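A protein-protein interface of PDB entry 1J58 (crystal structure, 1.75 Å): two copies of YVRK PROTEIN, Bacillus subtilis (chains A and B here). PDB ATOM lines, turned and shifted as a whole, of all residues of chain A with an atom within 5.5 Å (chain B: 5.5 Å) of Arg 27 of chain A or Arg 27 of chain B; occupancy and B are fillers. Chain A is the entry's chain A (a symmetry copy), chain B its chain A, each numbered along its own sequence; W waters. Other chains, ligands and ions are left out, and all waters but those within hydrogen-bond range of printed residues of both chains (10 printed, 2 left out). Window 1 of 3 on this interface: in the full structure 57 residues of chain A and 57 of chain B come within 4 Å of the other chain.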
ATOM      1  N   ASN A  24       7.732  -4.613 -26.119  1.00  0.00           N
ATOM      2  CA  ASN A  24       6.619  -3.951 -25.456  1.00  0.00           C
ATOM      3  C   ASN A  24       6.407  -2.615 -26.162  1.00  0.00           C
ATOM      4  O   ASN A  24       6.970  -1.594 -25.765  1.00  0.00           O
ATOM      5  CB  ASN A  24       6.953  -3.712 -23.985  1.00  0.00           C
ATOM      6  CG  ASN A  24       5.730  -3.388 -23.163  1.00  0.00           C
ATOM      7  OD1 ASN A  24       4.840  -2.671 -23.616  1.00  0.00           O
ATOM      8  ND2 ASN A  24       5.683  -3.908 -21.941  1.00  0.00           N
ATOM      9  N   ILE A  25       5.596  -2.625 -27.212  1.00  0.00           N
ATOM     10  CA  ILE A  25       5.352  -1.413 -27.979  1.00  0.00           C
ATOM     11  C   ILE A  25       4.664  -0.302 -27.183  1.00  0.00           C
ATOM     12  O   ILE A  25       4.980   0.872 -27.371  1.00  0.00           O
ATOM     13  CB  ILE A  25       4.533  -1.723 -29.261  1.00  0.00           C
ATOM     14  CG1 ILE A  25       4.672  -0.566 -30.251  1.00  0.00           C
ATOM     15  CG2 ILE A  25       3.075  -1.959 -28.917  1.00  0.00           C
ATOM     16  CD1 ILE A  25       6.093  -0.388 -30.761  1.00  0.00           C
ATOM     17  N   GLU A  26       3.741  -0.663 -26.291  1.00  0.00           N
ATOM     18  CA  GLU A  26       3.043   0.343 -25.492  1.00  0.00           C
ATOM     19  C   GLU A  26       4.012   1.139 -24.624  1.00  0.00           C
ATOM     20  O   GLU A  26       3.908   2.362 -24.534  1.00  0.00           O
ATOM     21  CB  GLU A  26       1.985  -0.294 -24.583  1.00  0.00           C
ATOM     22  CG  GLU A  26       0.809  -0.942 -25.298  1.00  0.00           C
ATOM     23  CD  GLU A  26       1.196  -2.214 -26.017  1.00  0.00           C
ATOM     24  OE1 GLU A  26       2.058  -2.955 -25.494  1.00  0.00           O
ATOM     25  OE2 GLU A  26       0.628  -2.483 -27.098  1.00  0.00           O
ATOM     26  N   ARG A  27       4.952   0.455 -23.981  1.00  0.00           N
ATOM     27  CA  ARG A  27       5.912   1.158 -23.139  1.00  0.00           C
ATOM     28  C   ARG A  27       6.891   1.954 -23.988  1.00  0.00           C
ATOM     29  O   ARG A  27       7.303   3.044 -23.600  1.00  0.00           O
ATOM     30  CB  ARG A  27       6.666   0.183 -22.222  1.00  0.00           C
ATOM     31  CG  ARG A  27       5.750  -0.519 -21.240  1.00  0.00           C
ATOM     32  CD  ARG A  27       6.474  -1.038 -20.003  1.00  0.00           C
ATOM     33  NE  ARG A  27       5.532  -1.731 -19.128  1.00  0.00           N
ATOM     34  CZ  ARG A  27       5.694  -1.901 -17.820  1.00  0.00           C
ATOM     35  NH1 ARG A  27       6.772  -1.431 -17.210  1.00  0.00           N
ATOM     36  NH2 ARG A  27       4.763  -2.534 -17.121  1.00  0.00           N
ATOM     37  N   ASP A  28       7.266   1.419 -25.148  1.00  0.00           N
ATOM     38  CA  ASP A  28       8.182   2.139 -26.023  1.00  0.00           C
ATOM     39  C   ASP A  28       7.550   3.466 -26.434  1.00  0.00           C
ATOM     40  O   ASP A  28       8.233   4.486 -26.512  1.00  0.00           O
ATOM     41  CB  ASP A  28       8.521   1.317 -27.272  1.00  0.00           C
ATOM     42  CG  ASP A  28       9.473   0.168 -26.980  1.00  0.00           C
ATOM     43  OD1 ASP A  28      10.132   0.186 -25.916  1.00  0.00           O
ATOM     44  OD2 ASP A  28       9.576  -0.748 -27.823  1.00  0.00           O
ATOM     45  N   ARG A  29       6.244   3.454 -26.691  1.00  0.00           N
ATOM     46  CA  ARG A  29       5.543   4.674 -27.080  1.00  0.00           C
ATOM     47  C   ARG A  29       5.515   5.679 -25.932  1.00  0.00           C
ATOM     48  O   ARG A  29       5.483   6.885 -26.165  1.00  0.00           O
ATOM     49  CB  ARG A  29       4.111   4.359 -27.523  1.00  0.00           C
ATOM     50  CG  ARG A  29       4.014   3.686 -28.882  1.00  0.00           C
ATOM     51  CD  ARG A  29       2.596   3.197 -29.131  1.00  0.00           C
ATOM     52  NE  ARG A  29       2.453   2.518 -30.415  1.00  0.00           N
ATOM     53  CZ  ARG A  29       1.566   1.555 -30.648  1.00  0.00           C
ATOM     54  NH1 ARG A  29       0.747   1.160 -29.679  1.00  0.00           N
ATOM     55  NH2 ARG A  29       1.493   0.989 -31.846  1.00  0.00           N
ATOM     56  N   GLN A  30       5.528   5.188 -24.696  1.00  0.00           N
ATOM     57  CA  GLN A  30       5.516   6.082 -23.539  1.00  0.00           C
ATOM     58  C   GLN A  30       6.909   6.637 -23.239  1.00  0.00           C
ATOM     59  O   GLN A  30       7.040   7.656 -22.562  1.00  0.00           O
ATOM     60  CB  GLN A  30       4.995   5.361 -22.291  1.00  0.00           C
ATOM     61  CG  GLN A  30       3.618   4.729 -22.442  1.00  0.00           C
ATOM     62  CD  GLN A  30       3.009   4.337 -21.104  1.00  0.00           C
ATOM     63  OE1 GLN A  30       3.725   4.056 -20.144  1.00  0.00           O
ATOM     64  NE2 GLN A  30       1.682   4.304 -21.042  1.00  0.00           N
ATOM     65  N   ASN A  31       7.941   5.970 -23.751  1.00  0.00           N
ATOM     66  CA  ASN A  31       9.323   6.387 -23.512  1.00  0.00           C
ATOM     67  C   ASN A  31      10.074   6.727 -24.801  1.00  0.00           C
ATOM     68  O   ASN A  31      11.115   6.141 -25.097  1.00  0.00           O
ATOM     69  CB  ASN A  31      10.075   5.277 -22.772  1.00  0.00           C
ATOM     70  CG  ASN A  31       9.442   4.934 -21.442  1.00  0.00           C
ATOM     71  OD1 ASN A  31       8.966   5.816 -20.728  1.00  0.00           O
ATOM     72  ND2 ASN A  31       9.446   3.652 -21.093  1.00  0.00           N
ATOM     73  N   LYS A  49      13.267   6.705 -12.714  1.00  0.00           N
ATOM     74  CA  LYS A  49      11.841   6.681 -13.019  1.00  0.00           C
ATOM     75  C   LYS A  49      11.152   5.377 -12.625  1.00  0.00           C
ATOM     76  O   LYS A  49      11.694   4.294 -12.820  1.00  0.00           O
ATOM     77  CB  LYS A  49      11.677   6.923 -14.523  1.00  0.00           C
ATOM     78  CG  LYS A  49      10.391   6.433 -15.163  1.00  0.00           C
ATOM     79  CD  LYS A  49      10.656   6.174 -16.649  1.00  0.00           C
ATOM     80  CE  LYS A  49       9.446   5.613 -17.375  1.00  0.00           C
ATOM     81  NZ  LYS A  49       8.352   6.610 -17.459  1.00  0.00           N
ATOM     82  N   SER A  51       6.876   3.796 -12.156  1.00  0.00           N
ATOM     83  CA  SER A  51       5.435   4.035 -12.167  1.00  0.00           C
ATOM     84  C   SER A  51       4.648   3.312 -11.079  1.00  0.00           C
ATOM     85  O   SER A  51       4.907   2.143 -10.793  1.00  0.00           O
ATOM     86  CB  SER A  51       4.867   3.636 -13.529  1.00  0.00           C
ATOM     87  OG  SER A  51       3.453   3.743 -13.533  1.00  0.00           O
ATOM     88  N   SER A  53       1.791   2.329 -11.389  1.00  0.00           N
ATOM     89  CA  SER A  53       1.051   1.281 -12.084  1.00  0.00           C
ATOM     90  C   SER A  53       1.840  -0.025 -12.118  1.00  0.00           C
ATOM     91  O   SER A  53       1.284  -1.089 -12.408  1.00  0.00           O
ATOM     92  CB  SER A  53       0.709   1.716 -13.512  1.00  0.00           C
ATOM     93  OG  SER A  53      -0.287   2.721 -13.508  1.00  0.00           O
ATOM     94  N   ASP A  54       3.133   0.062 -11.826  1.00  0.00           N
ATOM     95  CA  ASP A  54       3.985  -1.119 -11.807  1.00  0.00           C
ATOM     96  C   ASP A  54       4.173  -1.650 -10.388  1.00  0.00           C
ATOM     97  O   ASP A  54       5.132  -2.372 -10.110  1.00  0.00           O
ATOM     98  CB  ASP A  54       5.349  -0.816 -12.434  1.00  0.00           C
ATOM     99  CG  ASP A  54       5.287  -0.722 -13.950  1.00  0.00           C
ATOM    100  OD1 ASP A  54       4.614  -1.570 -14.568  1.00  0.00           O
ATOM    101  OD2 ASP A  54       5.918   0.186 -14.527  1.00  0.00           O
ATOM    102  N   ASP A 309       3.938   8.016 -12.382  1.00  0.00           N
ATOM    103  CA  ASP A 309       5.388   8.171 -12.321  1.00  0.00           C
ATOM    104  C   ASP A 309       6.050   8.967 -11.207  1.00  0.00           C
ATOM    105  O   ASP A 309       5.683  10.104 -10.896  1.00  0.00           O
ATOM    106  CB  ASP A 309       5.923   8.708 -13.650  1.00  0.00           C
ATOM    107  CG  ASP A 309       5.765   7.720 -14.778  1.00  0.00           C
ATOM    108  OD1 ASP A 309       5.337   6.578 -14.511  1.00  0.00           O
ATOM    109  OD2 ASP A 309       6.078   8.084 -15.928  1.00  0.00           O
ATOM    110  N   ASN B  24      -2.084   5.760 -15.481  1.00  0.00           N
ATOM    111  CA  ASN B  24      -1.466   5.142 -16.644  1.00  0.00           C
ATOM    112  C   ASN B  24      -2.284   3.899 -16.979  1.00  0.00           C
ATOM    113  O   ASN B  24      -1.987   2.802 -16.507  1.00  0.00           O
ATOM    114  CB  ASN B  24      -0.027   4.744 -16.324  1.00  0.00           C
ATOM    115  CG  ASN B  24       0.780   4.458 -17.566  1.00  0.00           C
ATOM    116  OD1 ASN B  24       0.279   3.866 -18.519  1.00  0.00           O
ATOM    117  ND2 ASN B  24       2.044   4.869 -17.559  1.00  0.00           N
ATOM    118  N   ILE B  25      -3.318   4.075 -17.792  1.00  0.00           N
ATOM    119  CA  ILE B  25      -4.186   2.962 -18.148  1.00  0.00           C
ATOM    120  C   ILE B  25      -3.482   1.850 -18.927  1.00  0.00           C
ATOM    121  O   ILE B  25      -3.778   0.674 -18.719  1.00  0.00           O
ATOM    122  CB  ILE B  25      -5.424   3.457 -18.943  1.00  0.00           C
ATOM    123  CG1 ILE B  25      -6.514   2.386 -18.915  1.00  0.00           C
ATOM    124  CG2 ILE B  25      -5.039   3.790 -20.373  1.00  0.00           C
ATOM    125  CD1 ILE B  25      -7.058   2.129 -17.518  1.00  0.00           C
ATOM    126  N   GLU B  26      -2.549   2.210 -19.809  1.00  0.00           N
ATOM    127  CA  GLU B  26      -1.831   1.202 -20.589  1.00  0.00           C
ATOM    128  C   GLU B  26      -1.051   0.249 -19.691  1.00  0.00           C
ATOM    129  O   GLU B  26      -1.068  -0.963 -19.903  1.00  0.00           O
ATOM    130  CB  GLU B  26      -0.855   1.846 -21.581  1.00  0.00           C
ATOM    131  CG  GLU B  26      -1.494   2.657 -22.699  1.00  0.00           C
ATOM    132  CD  GLU B  26      -2.103   3.950 -22.204  1.00  0.00           C
ATOM    133  OE1 GLU B  26      -1.528   4.562 -21.276  1.00  0.00           O
ATOM    134  OE2 GLU B  26      -3.147   4.363 -22.752  1.00  0.00           O
ATOM    135  N   ARG B  27      -0.363   0.787 -18.689  1.00  0.00           N
ATOM    136  CA  ARG B  27       0.400  -0.070 -17.790  1.00  0.00           C
ATOM    137  C   ARG B  27      -0.530  -0.870 -16.892  1.00  0.00           C
ATOM    138  O   ARG B  27      -0.246  -2.023 -16.577  1.00  0.00           O
ATOM    139  CB  ARG B  27       1.388   0.748 -16.948  1.00  0.00           C
ATOM    140  CG  ARG B  27       2.442   1.438 -17.791  1.00  0.00           C
ATOM    141  CD  ARG B  27       3.710   1.778 -17.015  1.00  0.00           C
ATOM    142  NE  ARG B  27       4.655   2.471 -17.887  1.00  0.00           N
ATOM    143  CZ  ARG B  27       5.971   2.509 -17.703  1.00  0.00           C
ATOM    144  NH1 ARG B  27       6.522   1.892 -16.667  1.00  0.00           N
ATOM    145  NH2 ARG B  27       6.736   3.156 -18.568  1.00  0.00           N
ATOM    146  N   ASP B  28      -1.643  -0.270 -16.478  1.00  0.00           N
ATOM    147  CA  ASP B  28      -2.591  -0.986 -15.635  1.00  0.00           C
ATOM    148  C   ASP B  28      -3.110  -2.211 -16.385  1.00  0.00           C
ATOM    149  O   ASP B  28      -3.287  -3.276 -15.797  1.00  0.00           O
ATOM    150  CB  ASP B  28      -3.767  -0.090 -15.232  1.00  0.00           C
ATOM    151  CG  ASP B  28      -3.388   0.940 -14.179  1.00  0.00           C
ATOM    152  OD1 ASP B  28      -2.339   0.769 -13.518  1.00  0.00           O
ATOM    153  OD2 ASP B  28      -4.149   1.915 -13.999  1.00  0.00           O
ATOM    154  N   ARG B  29      -3.346  -2.060 -17.687  1.00  0.00           N
ATOM    155  CA  ARG B  29      -3.831  -3.173 -18.496  1.00  0.00           C
ATOM    156  C   ARG B  29      -2.777  -4.270 -18.607  1.00  0.00           C
ATOM    157  O   ARG B  29      -3.115  -5.443 -18.748  1.00  0.00           O
ATOM    158  CB  ARG B  29      -4.225  -2.694 -19.897  1.00  0.00           C
ATOM    159  CG  ARG B  29      -5.517  -1.896 -19.942  1.00  0.00           C
ATOM    160  CD  ARG B  29      -5.702  -1.264 -21.312  1.00  0.00           C
ATOM    161  NE  ARG B  29      -6.920  -0.463 -21.402  1.00  0.00           N
ATOM    162  CZ  ARG B  29      -7.054   0.591 -22.201  1.00  0.00           C
ATOM    163  NH1 ARG B  29      -6.042   0.969 -22.975  1.00  0.00           N
ATOM    164  NH2 ARG B  29      -8.196   1.267 -22.229  1.00  0.00           N
ATOM    165  N   GLN B  30      -1.503  -3.895 -18.543  1.00  0.00           N
ATOM    166  CA  GLN B  30      -0.429  -4.884 -18.628  1.00  0.00           C
ATOM    167  C   GLN B  30      -0.199  -5.585 -17.289  1.00  0.00           C
ATOM    168  O   GLN B  30       0.383  -6.668 -17.245  1.00  0.00           O
ATOM    169  CB  GLN B  30       0.885  -4.234 -19.075  1.00  0.00           C
ATOM    170  CG  GLN B  30       0.810  -3.472 -20.391  1.00  0.00           C
ATOM    171  CD  GLN B  30       2.185  -3.149 -20.954  1.00  0.00           C
ATOM    172  OE1 GLN B  30       3.157  -3.019 -20.209  1.00  0.00           O
ATOM    173  NE2 GLN B  30       2.269  -3.004 -22.272  1.00  0.00           N
ATOM    174  N   ASN B  31      -0.664  -4.969 -16.203  1.00  0.00           N
ATOM    175  CA  ASN B  31      -0.483  -5.526 -14.863  1.00  0.00           C
ATOM    176  C   ASN B  31      -1.807  -5.815 -14.153  1.00  0.00           C
ATOM    177  O   ASN B  31      -2.064  -5.299 -13.066  1.00  0.00           O
ATOM    178  CB  ASN B  31       0.342  -4.558 -14.011  1.00  0.00           C
ATOM    179  CG  ASN B  31       1.706  -4.281 -14.602  1.00  0.00           C
ATOM    180  OD1 ASN B  31       2.346  -5.177 -15.151  1.00  0.00           O
ATOM    181  ND2 ASN B  31       2.167  -3.040 -14.481  1.00  0.00           N
ATOM    182  N   LYS B  49      10.189  -7.156 -10.898  1.00  0.00           N
ATOM    183  CA  LYS B  49       9.907  -6.978 -12.318  1.00  0.00           C
ATOM    184  C   LYS B  49      10.424  -5.659 -12.886  1.00  0.00           C
ATOM    185  O   LYS B  49      10.318  -4.615 -12.250  1.00  0.00           O
ATOM    186  CB  LYS B  49       8.390  -7.070 -12.512  1.00  0.00           C
ATOM    187  CG  LYS B  49       7.814  -6.412 -13.753  1.00  0.00           C
ATOM    188  CD  LYS B  49       6.353  -6.046 -13.475  1.00  0.00           C
ATOM    189  CE  LYS B  49       5.697  -5.318 -14.635  1.00  0.00           C
ATOM    190  NZ  LYS B  49       5.540  -6.203 -15.814  1.00  0.00           N
ATOM    191  N   SER B  51      11.092  -3.754 -17.000  1.00  0.00           N
ATOM    192  CA  SER B  51      11.079  -3.863 -18.456  1.00  0.00           C
ATOM    193  C   SER B  51      12.238  -3.173 -19.170  1.00  0.00           C
ATOM    194  O   SER B  51      12.623  -2.062 -18.805  1.00  0.00           O
ATOM    195  CB  SER B  51       9.766  -3.295 -18.995  1.00  0.00           C
ATOM    196  OG  SER B  51       9.773  -3.276 -20.413  1.00  0.00           O
ATOM    197  N   SER B  53      12.057  -1.918 -21.929  1.00  0.00           N
ATOM    198  CA  SER B  53      11.467  -0.750 -22.577  1.00  0.00           C
ATOM    199  C   SER B  53      11.538   0.478 -21.675  1.00  0.00           C
ATOM    200  O   SER B  53      11.351   1.610 -22.135  1.00  0.00           O
ATOM    201  CB  SER B  53      10.011  -1.024 -22.964  1.00  0.00           C
ATOM    202  OG  SER B  53       9.940  -1.933 -24.046  1.00  0.00           O
ATOM    203  N   ASP B  54      11.803   0.252 -20.392  1.00  0.00           N
ATOM    204  CA  ASP B  54      11.915   1.347 -19.438  1.00  0.00           C
ATOM    205  C   ASP B  54      13.372   1.730 -19.195  1.00  0.00           C
ATOM    206  O   ASP B  54      13.700   2.336 -18.174  1.00  0.00           O
ATOM    207  CB  ASP B  54      11.244   0.981 -18.110  1.00  0.00           C
ATOM    208  CG  ASP B  54       9.727   1.029 -18.190  1.00  0.00           C
ATOM    209  OD1 ASP B  54       9.196   1.985 -18.788  1.00  0.00           O
ATOM    210  OD2 ASP B  54       9.063   0.124 -17.646  1.00  0.00           O
ATOM    211  N   ASP B 309      10.534  -7.661 -20.305  1.00  0.00           N
ATOM    212  CA  ASP B 309      10.561  -7.948 -18.874  1.00  0.00           C
ATOM    213  C   ASP B 309      11.590  -8.896 -18.279  1.00  0.00           C
ATOM    214  O   ASP B 309      11.805 -10.019 -18.745  1.00  0.00           O
ATOM    215  CB  ASP B 309       9.182  -8.410 -18.397  1.00  0.00           C
ATOM    216  CG  ASP B 309       8.149  -7.315 -18.473  1.00  0.00           C
ATOM    217  OD1 ASP B 309       8.522  -6.167 -18.795  1.00  0.00           O
ATOM    218  OD2 ASP B 309       6.967  -7.600 -18.201  1.00  0.00           O
HETATM  219  O   HOH W   1      12.321   3.462 -15.930  1.00  0.00           O
HETATM  220  O   HOH W   2      10.396  -4.310 -25.224  1.00  0.00           O
HETATM  221  O   HOH W   3       7.286  -3.568 -11.570  1.00  0.00           O
HETATM  222  O   HOH W   4       8.140  -5.485 -21.406  1.00  0.00           O
HETATM  223  O   HOH W   5       1.264  -5.196 -24.458  1.00  0.00           O
HETATM  224  O   HOH W   6      11.788   2.026 -24.877  1.00  0.00           O
HETATM  225  O   HOH W   7      -1.491  -1.296 -12.026  1.00  0.00           O
HETATM  226  O   HOH W   8       2.682   6.168 -14.968  1.00  0.00           O
HETATM  227  O   HOH W   9      -0.287   6.762 -21.860  1.00  0.00           O
HETATM  228  O   HOH W  10      -1.256   5.144 -12.849  1.00  0.00           O
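Along chain A the printed residues that touch a printed residue of chain B span positions 24 to 54.
Among the printed residues, 27 pairs touch across the chains.
Of chain B, only Arg 27, Gln 30, Asn 31, Lys 49, Ser 51, Ser 53 and Asp 54 come within 4 Å of Arg 27 of chain A.
Arg 27 of chain B touches just these residues of chain A: Arg 27 (3.4 Å), Gln 30 (2.9 Å), Asn 31 (3.7 Å), Lys 49 (3.8 Å), Ser 51 (3.95 Å), Ser 53 (3.6 Å) and Asp 54 (2.8 Å).
Of the printed residues of chain A, Glu 26 of chain B touches Gln 30.
Printed residues of chain B within 4 Å of Gln 30 of chain A: Asn 24, Glu 26 and Arg 27.
Of the printed residues of chain A, Gln 30 of chain B touches Asn 24 (2.9 Å), Glu 26 (3.2 Å) and Arg 27 (2.9 Å).
Of the printed residues of chain B, Asp 28 of chain A touches Ser 53 (2.8 Å).
Printed residues of chain B within 4 Å of Ser 53 of chain A: Asn 24 (3.4 Å), Arg 27 (3.6 Å), Asp 28 (2.8 Å) and Asn 31 (3.0 Å).
Arg 29 of chain B touches none of the printed residues of chain A.
Asp 309 of chain B touches none of the printed residues of chain A.
The nearest residue of chain B that does not touch Arg 27 of chain A is Asp 309 of chain B (5.2 Å).
NH2 of Arg 27 of chain B is in salt-bridge range of OD1 of Asp 54 of chain B, 2.7 Å away.
The side-chain amino group (NZ) of Lys 49 of chain B sits close to the side-chain amide oxygen (OD1) of Asn 31 of chain B.
The side-chain amino group (NZ) of Lys 49 of chain B lies within salt-bridge range of the side-chain carboxylate (OD2) of Asp 309 of chain B (3.1 Å).
OG of Ser 51 of chain B lies close to N of Ser 53 of chain B.
NZ of Lys 49 of chain A lies close to OD1 of Asn 31 of chain A.
The side-chain hydroxyl of Ser 51 of chain A sits close to the backbone NH of Ser 53 of chain A.
Asn 24 of chain A touches Ser 53 of chain B, and with the chains exchanged Ser 53 of chain A touches Asn 24 of chain B.
Arg 27 of chain A touches Lys 49 of chain B, and with the chains exchanged Lys 49 of chain A touches Arg 27 of chain B.
Asn 31 of chain A touches Ser 53 of chain B, and with the chains exchanged Ser 53 of chain A touches Asn 31 of chain B.
Lys 49 of chain A touches Asp 54 of chain B, and with the chains exchanged Asp 54 of chain A touches Lys 49 of chain B.
Positions printed for both chains: 24, 25, 26, 27, 28, 29, 30, 31, 49, 51, 53, 54 and 309.
Of the 27 pairs that touch across the chains among the printed residues, 27 have their exchanged pair printed and touching as well.
Water W9 bridges the side-chain carboxylate (OE1) of Glu 26 of chain B and the side-chain amide nitrogen (NE2) of Gln 30 of chain A.
Water W5 bridges OE1 of Glu 26 of chain A and NE2 of Gln 30 of chain B.
Water W7 bridges OD1 of Asp 28 of chain B (2.7 Å) and O of Ser 53 of chain A (2.8 Å).
Water W2 lies within hydrogen-bond range of the side-chain hydroxyl of Ser 53 of chain B (2.7 Å) and the backbone NH of Asn 24 of chain A (2.8 Å).
Water W4 lies within hydrogen-bond range of the side-chain carboxylate of Asp 309 of chain B (2.7 Å), the side-chain hydroxyl of Ser 51 of chain B (2.9 Å) and the side-chain amide nitrogen of Asn 24 of chain A (3.0 Å).
Water W8 lies within hydrogen-bond range of the side-chain carboxylate (OD1) of Asp 309 of chain A (2.7 Å), the side-chain hydroxyl (OG) of Ser 51 of chain A (2.9 Å) and the side-chain amide nitrogen (ND2) of Asn 24 of chain B (3.0 Å).
The side-chain amide nitrogen of Gln 30 of chain A is in hydrogen-bond range of the side-chain amide oxygen of Asn 24 of chain B, 2.9 Å away.
The backbone carbonyl oxygen (O) of Asn 24 of chain B lies within hydrogen-bond range of the side-chain hydroxyl (OG) of Ser 53 of chain A, at 3.4 Å.
OE1 of Glu 26 of chain B lies within hydrogen-bond range of NE2 of Gln 30 of chain A.
The side-chain amide oxygen (OE1) of Gln 30 of chain A lies within hydrogen-bond range of the guanidinium group (NE) of Arg 27 of chain B (2.9 Å).
The side-chain carboxylate (OD2) of Asp 54 of chain A lies within salt-bridge range of the guanidinium group (NH1) of Arg 27 of chain B (2.8 Å).
The side-chain carboxylate (OD1) of Asp 28 of chain B lies within hydrogen-bond range of the side-chain hydroxyl (OG) of Ser 53 of chain A (2.8 Å).
The side-chain amide nitrogen of Gln 30 of chain B lies within hydrogen-bond range of the side-chain amide oxygen of Asn 24 of chain A (2.9 Å).
The side-chain carboxylate (OE1) of Glu 26 of chain A sits at hydrogen-bond distance from the side-chain amide nitrogen (NE2) of Gln 30 of chain B (3.2 Å).
OE1 of Gln 30 of chain B lies within hydrogen-bond range of NE of Arg 27 of chain A (2.9 Å).
The side-chain amide nitrogen of Asn 31 of chain B is in hydrogen-bond range of the backbone carbonyl oxygen of Ser 53 of chain A, 3.0 Å away.
The side-chain amide nitrogen of Asn 31 of chain B is in hydrogen-bond range of the side-chain carboxylate of Asp 54 of chain A (2.9 Å).
The backbone carbonyl oxygen of Asn 24 of chain A lies within hydrogen-bond range of the side-chain hydroxyl of Ser 53 of chain B (3.4 Å).
The side-chain hydroxyl of Ser 53 of chain B lies within hydrogen-bond range of the side-chain carboxylate of Asp 28 of chain A (2.8 Å).
O of Ser 53 of chain B lies within hydrogen-bond range of ND2 of Asn 31 of chain A.
OD2 of Asp 54 of chain B is in salt-bridge range of NH1 of Arg 27 of chain A, at 2.8 Å.
The side-chain carboxylate (OD1) of Asp 54 of chain B is in hydrogen-bond range of the side-chain amide nitrogen (ND2) of Asn 31 of chain A (2.9 Å).
The guanidinium group (NH1) of Arg 27 of chain A lies close to the guanidinium group (NH1) of Arg 27 of chain B, at 3.4 Å.
Among the printed residues, pairs that only touch across the chains: Arg 27 of chain A with Asn 31 of chain B (3.7 Å), Arg 27 of chain A with Lys 49 of chain B (3.8 Å), Arg 27 of chain A with Ser 51 of chain B (3.95 Å), Arg 27 of chain A with Ser 53 of chain B (3.6 Å), Asn 31 of chain A with Arg 27 of chain B (3.7 Å), Lys 49 of chain A with Arg 27 of chain B (3.8 Å), Lys 49 of chain A with Asp 54 of chain B (3.9 Å), Ser 51 of chain A with Arg 27 of chain B (3.95 Å), Ser 53 of chain A with Arg 27 of chain B (3.6 Å) and Asp 54 of chain A with Lys 49 of chain B (3.9 Å).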
